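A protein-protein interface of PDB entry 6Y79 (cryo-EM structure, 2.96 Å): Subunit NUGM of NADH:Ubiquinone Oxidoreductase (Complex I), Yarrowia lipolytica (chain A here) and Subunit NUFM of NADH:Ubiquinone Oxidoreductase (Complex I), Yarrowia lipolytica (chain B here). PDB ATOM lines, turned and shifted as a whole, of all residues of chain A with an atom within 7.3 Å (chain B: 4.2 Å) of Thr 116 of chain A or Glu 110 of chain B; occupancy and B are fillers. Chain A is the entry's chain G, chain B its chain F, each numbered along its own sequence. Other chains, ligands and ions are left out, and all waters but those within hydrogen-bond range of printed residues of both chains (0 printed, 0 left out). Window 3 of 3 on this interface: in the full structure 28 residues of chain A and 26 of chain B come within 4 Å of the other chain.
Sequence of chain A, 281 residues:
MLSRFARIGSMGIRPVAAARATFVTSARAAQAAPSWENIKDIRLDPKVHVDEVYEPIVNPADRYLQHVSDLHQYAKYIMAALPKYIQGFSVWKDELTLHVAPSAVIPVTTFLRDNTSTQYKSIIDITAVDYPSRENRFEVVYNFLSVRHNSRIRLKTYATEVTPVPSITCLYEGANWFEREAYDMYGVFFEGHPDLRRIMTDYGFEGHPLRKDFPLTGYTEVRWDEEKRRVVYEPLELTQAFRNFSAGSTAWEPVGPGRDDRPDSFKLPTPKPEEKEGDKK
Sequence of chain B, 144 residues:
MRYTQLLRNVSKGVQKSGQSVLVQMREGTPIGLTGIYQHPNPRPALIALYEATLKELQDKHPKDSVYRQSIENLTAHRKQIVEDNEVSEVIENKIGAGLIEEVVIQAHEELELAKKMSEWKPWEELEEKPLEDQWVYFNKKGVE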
ATOM      1  N   PHE A 111     -24.661 -23.642   9.082  1.00  0.00           N
ATOM      2  CA  PHE A 111     -23.472 -23.469   9.908  1.00  0.00           C
ATOM      3  C   PHE A 111     -22.352 -22.797   9.126  1.00  0.00           C
ATOM      4  O   PHE A 111     -21.786 -21.792   9.576  1.00  0.00           O
ATOM      5  CB  PHE A 111     -23.020 -24.825  10.437  1.00  0.00           C
ATOM      6  CG  PHE A 111     -21.814 -24.762  11.309  1.00  0.00           C
ATOM      7  CD1 PHE A 111     -21.901 -24.259  12.591  1.00  0.00           C
ATOM      8  CD2 PHE A 111     -20.592 -25.215  10.851  1.00  0.00           C
ATOM      9  CE1 PHE A 111     -20.789 -24.205  13.396  1.00  0.00           C
ATOM     10  CE2 PHE A 111     -19.480 -25.166  11.653  1.00  0.00           C
ATOM     11  CZ  PHE A 111     -19.579 -24.659  12.927  1.00  0.00           C
ATOM     12  N   LEU A 112     -22.116 -23.262   7.893  1.00  0.00           N
ATOM     13  CA  LEU A 112     -21.049 -22.699   7.076  1.00  0.00           C
ATOM     14  C   LEU A 112     -21.365 -21.282   6.641  1.00  0.00           C
ATOM     15  O   LEU A 112     -20.446 -20.503   6.378  1.00  0.00           O
ATOM     16  CB  LEU A 112     -20.791 -23.575   5.853  1.00  0.00           C
ATOM     17  CG  LEU A 112     -20.253 -24.983   6.086  1.00  0.00           C
ATOM     18  CD1 LEU A 112     -20.186 -25.714   4.772  1.00  0.00           C
ATOM     19  CD2 LEU A 112     -18.900 -24.959   6.748  1.00  0.00           C
ATOM     20  N   ARG A 113     -22.641 -20.910   6.588  1.00  0.00           N
ATOM     21  CA  ARG A 113     -22.920 -19.527   6.241  1.00  0.00           C
ATOM     22  C   ARG A 113     -22.717 -18.622   7.449  1.00  0.00           C
ATOM     23  O   ARG A 113     -22.317 -17.465   7.305  1.00  0.00           O
ATOM     24  CB  ARG A 113     -24.338 -19.400   5.679  1.00  0.00           C
ATOM     25  CG  ARG A 113     -24.704 -18.016   5.167  1.00  0.00           C
ATOM     26  CD  ARG A 113     -26.079 -17.967   4.506  1.00  0.00           C
ATOM     27  NE  ARG A 113     -27.187 -18.309   5.401  1.00  0.00           N
ATOM     28  CZ  ARG A 113     -27.775 -17.470   6.255  1.00  0.00           C
ATOM     29  NH1 ARG A 113     -28.777 -17.894   7.015  1.00  0.00           N
ATOM     30  NH2 ARG A 113     -27.342 -16.224   6.385  1.00  0.00           N
ATOM     31  N   ASP A 114     -22.938 -19.143   8.653  1.00  0.00           N
ATOM     32  CA  ASP A 114     -23.317 -18.255   9.746  1.00  0.00           C
ATOM     33  C   ASP A 114     -22.334 -18.216  10.893  1.00  0.00           C
ATOM     34  O   ASP A 114     -22.322 -17.234  11.643  1.00  0.00           O
ATOM     35  CB  ASP A 114     -24.693 -18.634  10.291  1.00  0.00           C
ATOM     36  CG  ASP A 114     -25.747 -18.546   9.239  1.00  0.00           C
ATOM     37  OD1 ASP A 114     -25.578 -17.705   8.333  1.00  0.00           O
ATOM     38  OD2 ASP A 114     -26.714 -19.325   9.266  1.00  0.00           O
ATOM     39  N   ASN A 115     -21.562 -19.274  11.093  1.00  0.00           N
ATOM     40  CA  ASN A 115     -20.533 -19.241  12.113  1.00  0.00           C
ATOM     41  C   ASN A 115     -19.483 -18.213  11.730  1.00  0.00           C
ATOM     42  O   ASN A 115     -19.077 -18.119  10.571  1.00  0.00           O
ATOM     43  CB  ASN A 115     -19.894 -20.615  12.286  1.00  0.00           C
ATOM     44  CG  ASN A 115     -18.977 -20.681  13.489  1.00  0.00           C
ATOM     45  OD1 ASN A 115     -18.972 -19.789  14.337  1.00  0.00           O
ATOM     46  ND2 ASN A 115     -18.192 -21.743  13.571  1.00  0.00           N
ATOM     47  N   THR A 116     -19.074 -17.422  12.719  1.00  0.00           N
ATOM     48  CA  THR A 116     -18.081 -16.376  12.535  1.00  0.00           C
ATOM     49  C   THR A 116     -16.741 -16.935  12.094  1.00  0.00           C
ATOM     50  O   THR A 116     -15.975 -16.237  11.428  1.00  0.00           O
ATOM     51  CB  THR A 116     -17.911 -15.650  13.842  1.00  0.00           C
ATOM     52  OG1 THR A 116     -17.914 -16.645  14.869  1.00  0.00           O
ATOM     53  CG2 THR A 116     -19.070 -14.728  14.089  1.00  0.00           C
ATOM     54  N   SER A 117     -16.442 -18.180  12.457  1.00  0.00           N
ATOM     55  CA  SER A 117     -15.213 -18.819  12.013  1.00  0.00           C
ATOM     56  C   SER A 117     -15.299 -19.257  10.556  1.00  0.00           C
ATOM     57  O   SER A 117     -14.276 -19.292   9.865  1.00  0.00           O
ATOM     58  CB  SER A 117     -14.906 -20.004  12.926  1.00  0.00           C
ATOM     59  OG  SER A 117     -13.745 -20.692  12.512  1.00  0.00           O
ATOM     60  N   THR A 118     -16.490 -19.599  10.068  1.00  0.00           N
ATOM     61  CA  THR A 118     -16.604 -20.125   8.715  1.00  0.00           C
ATOM     62  C   THR A 118     -16.944 -19.044   7.698  1.00  0.00           C
ATOM     63  O   THR A 118     -16.107 -18.712   6.855  1.00  0.00           O
ATOM     64  CB  THR A 118     -17.664 -21.225   8.677  1.00  0.00           C
ATOM     65  OG1 THR A 118     -18.958 -20.660   8.909  1.00  0.00           O
ATOM     66  CG2 THR A 118     -17.386 -22.263   9.739  1.00  0.00           C
ATOM     67  N   GLN A 119     -18.146 -18.469   7.813  1.00  0.00           N
ATOM     68  CA  GLN A 119     -18.628 -17.344   6.999  1.00  0.00           C
ATOM     69  C   GLN A 119     -18.543 -17.603   5.497  1.00  0.00           C
ATOM     70  O   GLN A 119     -18.192 -16.721   4.717  1.00  0.00           O
ATOM     71  CB  GLN A 119     -17.891 -16.059   7.350  1.00  0.00           C
ATOM     72  CG  GLN A 119     -18.318 -15.452   8.644  1.00  0.00           C
ATOM     73  CD  GLN A 119     -17.540 -14.214   8.954  1.00  0.00           C
ATOM     74  OE1 GLN A 119     -16.905 -13.635   8.078  1.00  0.00           O
ATOM     75  NE2 GLN A 119     -17.557 -13.807  10.210  1.00  0.00           N
ATOM     76  N   SER A 146     -15.477 -18.185   1.253  1.00  0.00           N
ATOM     77  CA  SER A 146     -15.445 -17.126   2.248  1.00  0.00           C
ATOM     78  C   SER A 146     -14.509 -16.045   1.737  1.00  0.00           C
ATOM     79  O   SER A 146     -13.284 -16.227   1.729  1.00  0.00           O
ATOM     80  CB  SER A 146     -14.973 -17.664   3.594  1.00  0.00           C
ATOM     81  OG  SER A 146     -14.416 -16.635   4.387  1.00  0.00           O
ATOM     82  N   ARG A 148     -14.230 -13.286   3.243  1.00  0.00           N
ATOM     83  CA  ARG A 148     -13.648 -12.678   4.431  1.00  0.00           C
ATOM     84  C   ARG A 148     -12.311 -13.311   4.769  1.00  0.00           C
ATOM     85  O   ARG A 148     -11.279 -12.634   4.831  1.00  0.00           O
ATOM     86  CB  ARG A 148     -14.594 -12.823   5.614  1.00  0.00           C
ATOM     87  CG  ARG A 148     -14.015 -12.214   6.858  1.00  0.00           C
ATOM     88  CD  ARG A 148     -13.915 -10.736   6.632  1.00  0.00           C
ATOM     89  NE  ARG A 148     -15.224 -10.243   6.247  1.00  0.00           N
ATOM     90  CZ  ARG A 148     -16.047  -9.682   7.105  1.00  0.00           C
ATOM     91  NH1 ARG A 148     -15.636  -9.541   8.345  1.00  0.00           N
ATOM     92  NH2 ARG A 148     -17.245  -9.260   6.737  1.00  0.00           N
ATOM     93  N   HIS A 149     -12.316 -14.610   5.013  1.00  0.00           N
ATOM     94  CA  HIS A 149     -11.129 -15.327   5.428  1.00  0.00           C
ATOM     95  C   HIS A 149     -10.326 -15.861   4.259  1.00  0.00           C
ATOM     96  O   HIS A 149      -9.289 -16.488   4.495  1.00  0.00           O
ATOM     97  CB  HIS A 149     -11.517 -16.474   6.359  1.00  0.00           C
ATOM     98  CG  HIS A 149     -12.280 -16.026   7.563  1.00  0.00           C
ATOM     99  ND1 HIS A 149     -13.630 -16.246   7.718  1.00  0.00           N
ATOM    100  CD2 HIS A 149     -11.887 -15.325   8.649  1.00  0.00           C
ATOM    101  CE1 HIS A 149     -14.030 -15.724   8.862  1.00  0.00           C
ATOM    102  NE2 HIS A 149     -12.990 -15.160   9.448  1.00  0.00           N
ATOM    103  N   THR B  53     -26.485 -13.769  22.993  1.00  0.00           N
ATOM    104  CA  THR B  53     -25.882 -14.998  22.501  1.00  0.00           C
ATOM    105  C   THR B  53     -25.418 -15.874  23.657  1.00  0.00           C
ATOM    106  O   THR B  53     -25.751 -17.061  23.704  1.00  0.00           O
ATOM    107  CB  THR B  53     -24.744 -14.678  21.531  1.00  0.00           C
ATOM    108  OG1 THR B  53     -25.252 -13.909  20.446  1.00  0.00           O
ATOM    109  CG2 THR B  53     -24.131 -15.959  21.002  1.00  0.00           C
ATOM    110  N   ILE B  71     -18.166 -21.240  21.033  1.00  0.00           N
ATOM    111  CA  ILE B  71     -18.839 -19.958  20.826  1.00  0.00           C
ATOM    112  C   ILE B  71     -18.968 -19.183  22.144  1.00  0.00           C
ATOM    113  O   ILE B  71     -18.975 -17.943  22.131  1.00  0.00           O
ATOM    114  CB  ILE B  71     -20.182 -20.173  20.104  1.00  0.00           C
ATOM    115  CG1 ILE B  71     -19.936 -21.030  18.863  1.00  0.00           C
ATOM    116  CG2 ILE B  71     -20.812 -18.845  19.683  1.00  0.00           C
ATOM    117  CD1 ILE B  71     -21.011 -20.981  17.803  1.00  0.00           C
ATOM    118  N   LEU B  74     -15.529 -17.565  22.290  1.00  0.00           N
ATOM    119  CA  LEU B  74     -15.392 -16.614  21.198  1.00  0.00           C
ATOM    120  C   LEU B  74     -16.146 -15.321  21.475  1.00  0.00           C
ATOM    121  O   LEU B  74     -15.583 -14.223  21.352  1.00  0.00           O
ATOM    122  CB  LEU B  74     -15.897 -17.258  19.922  1.00  0.00           C
ATOM    123  CG  LEU B  74     -15.793 -16.358  18.718  1.00  0.00           C
ATOM    124  CD1 LEU B  74     -14.340 -16.082  18.454  1.00  0.00           C
ATOM    125  CD2 LEU B  74     -16.388 -17.144  17.617  1.00  0.00           C
ATOM    126  N   THR B  75     -17.432 -15.431  21.834  1.00  0.00           N
ATOM    127  CA  THR B  75     -18.206 -14.246  22.171  1.00  0.00           C
ATOM    128  C   THR B  75     -17.710 -13.594  23.454  1.00  0.00           C
ATOM    129  O   THR B  75     -17.788 -12.370  23.570  1.00  0.00           O
ATOM    130  CB  THR B  75     -19.689 -14.613  22.271  1.00  0.00           C
ATOM    131  OG1 THR B  75     -20.027 -15.491  21.194  1.00  0.00           O
ATOM    132  CG2 THR B  75     -20.568 -13.382  22.167  1.00  0.00           C
ATOM    133  N   GLN B 106     -22.553  -9.802  11.919  1.00  0.00           N
ATOM    134  CA  GLN B 106     -22.039 -11.137  12.221  1.00  0.00           C
ATOM    135  C   GLN B 106     -22.486 -11.633  13.588  1.00  0.00           C
ATOM    136  O   GLN B 106     -22.749 -12.828  13.757  1.00  0.00           O
ATOM    137  CB  GLN B 106     -20.523 -11.139  12.160  1.00  0.00           C
ATOM    138  CG  GLN B 106     -19.996 -10.948  10.796  1.00  0.00           C
ATOM    139  CD  GLN B 106     -18.514 -10.790  10.792  1.00  0.00           C
ATOM    140  OE1 GLN B 106     -17.882 -10.661  11.835  1.00  0.00           O
ATOM    141  NE2 GLN B 106     -17.943 -10.817   9.617  1.00  0.00           N
ATOM    142  N   ALA B 107     -22.531 -10.745  14.585  1.00  0.00           N
ATOM    143  CA  ALA B 107     -22.986 -11.148  15.914  1.00  0.00           C
ATOM    144  C   ALA B 107     -24.469 -11.488  15.913  1.00  0.00           C
ATOM    145  O   ALA B 107     -24.896 -12.438  16.582  1.00  0.00           O
ATOM    146  CB  ALA B 107     -22.695 -10.044  16.923  1.00  0.00           C
ATOM    147  N   HIS B 108     -25.258 -10.747  15.136  1.00  0.00           N
ATOM    148  CA  HIS B 108     -26.648 -11.118  14.906  1.00  0.00           C
ATOM    149  C   HIS B 108     -26.759 -12.473  14.225  1.00  0.00           C
ATOM    150  O   HIS B 108     -27.653 -13.278  14.542  1.00  0.00           O
ATOM    151  CB  HIS B 108     -27.293 -10.048  14.053  1.00  0.00           C
ATOM    152  CG  HIS B 108     -28.695 -10.345  13.648  1.00  0.00           C
ATOM    153  ND1 HIS B 108     -29.764 -10.133  14.485  1.00  0.00           N
ATOM    154  CD2 HIS B 108     -29.208 -10.797  12.481  1.00  0.00           C
ATOM    155  CE1 HIS B 108     -30.878 -10.458  13.855  1.00  0.00           C
ATOM    156  NE2 HIS B 108     -30.569 -10.865  12.639  1.00  0.00           N
ATOM    157  N   GLU B 109     -25.846 -12.746  13.291  1.00  0.00           N
ATOM    158  CA  GLU B 109     -25.930 -13.980  12.529  1.00  0.00           C
ATOM    159  C   GLU B 109     -25.564 -15.187  13.383  1.00  0.00           C
ATOM    160  O   GLU B 109     -26.230 -16.227  13.311  1.00  0.00           O
ATOM    161  CB  GLU B 109     -25.046 -13.879  11.293  1.00  0.00           C
ATOM    162  CG  GLU B 109     -25.326 -14.999  10.367  1.00  0.00           C
ATOM    163  CD  GLU B 109     -26.760 -14.948   9.870  1.00  0.00           C
ATOM    164  OE1 GLU B 109     -27.240 -13.857   9.499  1.00  0.00           O
ATOM    165  OE2 GLU B 109     -27.441 -15.991   9.963  1.00  0.00           O
ATOM    166  N   GLU B 110     -24.536 -15.058  14.224  1.00  0.00           N
ATOM    167  CA  GLU B 110     -24.210 -16.145  15.143  1.00  0.00           C
ATOM    168  C   GLU B 110     -25.276 -16.308  16.223  1.00  0.00           C
ATOM    169  O   GLU B 110     -25.476 -17.423  16.715  1.00  0.00           O
ATOM    170  CB  GLU B 110     -22.830 -15.936  15.769  1.00  0.00           C
ATOM    171  CG  GLU B 110     -22.747 -14.809  16.766  1.00  0.00           C
ATOM    172  CD  GLU B 110     -21.471 -14.802  17.563  1.00  0.00           C
ATOM    173  OE1 GLU B 110     -21.208 -15.799  18.263  1.00  0.00           O
ATOM    174  OE2 GLU B 110     -20.736 -13.794  17.497  1.00  0.00           O
ATOM    175  N   LEU B 111     -26.009 -15.236  16.561  1.00  0.00           N
ATOM    176  CA  LEU B 111     -27.117 -15.372  17.504  1.00  0.00           C
ATOM    177  C   LEU B 111     -28.245 -16.216  16.920  1.00  0.00           C
ATOM    178  O   LEU B 111     -28.761 -17.124  17.586  1.00  0.00           O
ATOM    179  CB  LEU B 111     -27.634 -13.995  17.915  1.00  0.00           C
ATOM    180  CG  LEU B 111     -28.911 -13.998  18.762  1.00  0.00           C
ATOM    181  CD1 LEU B 111     -28.715 -14.730  20.080  1.00  0.00           C
ATOM    182  CD2 LEU B 111     -29.365 -12.595  19.019  1.00  0.00           C
ATOM    183  N   GLU B 112     -28.640 -15.943  15.675  1.00  0.00           N
ATOM    184  CA  GLU B 112     -29.723 -16.746  15.105  1.00  0.00           C
ATOM    185  C   GLU B 112     -29.252 -18.155  14.732  1.00  0.00           C
ATOM    186  O   GLU B 112     -30.048 -19.105  14.780  1.00  0.00           O
ATOM    187  CB  GLU B 112     -30.360 -16.018  13.916  1.00  0.00           C
ATOM    188  CG  GLU B 112     -31.577 -16.726  13.290  1.00  0.00           C
ATOM    189  CD  GLU B 112     -32.753 -16.936  14.248  1.00  0.00           C
ATOM    190  OE1 GLU B 112     -32.946 -16.131  15.185  1.00  0.00           O
ATOM    191  OE2 GLU B 112     -33.487 -17.932  14.066  1.00  0.00           O
ATOM    192  N   LEU B 113     -27.959 -18.327  14.435  1.00  0.00           N
ATOM    193  CA  LEU B 113     -27.399 -19.668  14.274  1.00  0.00           C
ATOM    194  C   LEU B 113     -27.493 -20.461  15.568  1.00  0.00           C
ATOM    195  O   LEU B 113     -27.892 -21.636  15.571  1.00  0.00           O
ATOM    196  CB  LEU B 113     -25.939 -19.579  13.834  1.00  0.00           C
ATOM    197  CG  LEU B 113     -25.271 -20.939  13.637  1.00  0.00           C
ATOM    198  CD1 LEU B 113     -25.855 -21.609  12.425  1.00  0.00           C
ATOM    199  CD2 LEU B 113     -23.772 -20.817  13.517  1.00  0.00           C
ATOM    200  N   ALA B 114     -27.130 -19.825  16.681  1.00  0.00           N
ATOM    201  CA  ALA B 114     -27.208 -20.470  17.980  1.00  0.00           C
ATOM    202  C   ALA B 114     -28.646 -20.752  18.393  1.00  0.00           C
ATOM    203  O   ALA B 114     -28.897 -21.747  19.074  1.00  0.00           O
ATOM    204  CB  ALA B 114     -26.491 -19.602  19.011  1.00  0.00           C
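The side-chain carboxylate (OD1) of Asp 114 of chain A lies close to the side-chain carboxylate (OE2) of Glu 109 of chain B (3.0 Å). The side-chain carboxylate of Glu 109 of chain B is in salt-bridge range of the guanidinium group of Arg 113 of chain A, 3.6 Å away. NE2 of Gln 106 of chain B sits close to NH1 of Arg 148 of chain A (2.9 Å). The side-chain amide nitrogen of Gln 106 of chain B lies close to the side-chain amide nitrogen of Gln 119 of chain A (3.1 Å).
Leu 113 of chain B touches Phe 111 of chain A (CD1 to CA, 3.9 Å). Asp 114 of chain A touches Leu 113 of chain B. Leu 113 of chain B touches Asn 115 of chain A (CD2 to N, 3.6 Å). Leu 74 of chain B touches Thr 116 of chain A (CD2 to OG1, 3.2 Å). Thr 116 of chain A touches Glu 110 of chain B (CG2 to OE2, 3.9 Å).
O of Thr 116 of chain A lies within hydrogen-bond range of NE2 of Gln 119 of chain A, 3.1 Å away. OE1 of Glu 110 of chain B lies within hydrogen-bond range of OG1 of Thr 75 of chain B (3.2 Å). N of Gln 119 of chain A lies within hydrogen-bond range of O of Leu 112 of chain A, at 3.4 Å. The backbone carbonyl oxygen (O) of Phe 111 of chain A lies within hydrogen-bond range of the side-chain hydroxyl (OG1) of Thr 118 of chain A (3.1 Å). The guanidinium group (NH2) of Arg 113 of chain A lies within salt-bridge range of the side-chain carboxylate (OD1) of Asp 114 of chain A. O of Asn 115 of chain A lies within hydrogen-bond range of OG1 of Thr 118 of chain A.
Of the printed residues of chain B, Thr 116 of chain A touches Leu 74 and Glu 110. Printed residues of chain B within 4 Å of Arg 148 of chain A: Gln 106. Ile 71 of chain B touches none of the printed residues of chain A. Of the printed residues of chain A, Gln 106 of chain B touches Gln 119 and Arg 148. His 108 of chain B touches none of the printed residues of chain A. The nearest printed residue of chain B that does not touch Thr 116 of chain A is Gln 106 of chain B (4.2 Å). The nearest residue of chain A that does not touch Glu 110 of chain B is Asp 114 of chain A (4.04 Å). The nearest printed residue of chain B that does not touch Arg 113 of chain A is Leu 113 of chain B (6.5 Å).
Printed residues of chain A that touch a printed residue of chain B: Phe 111, Arg 113, Asp 114, Asn 115, Thr 116, Gln 119 and Arg 148. Of the 13 printed residues of chain B, 5 touch a printed residue of chain A. Along chain B the printed residues that touch a printed residue of chain A span positions 74 to 113. Among the printed residues, 9 pairs touch across the chains. Among the printed residues, Asp or Glu carboxylates within 4 Å of a Lys or Arg side-chain nitrogen of the other chain: Arg 113 of chain A with Glu 109 of chain B.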
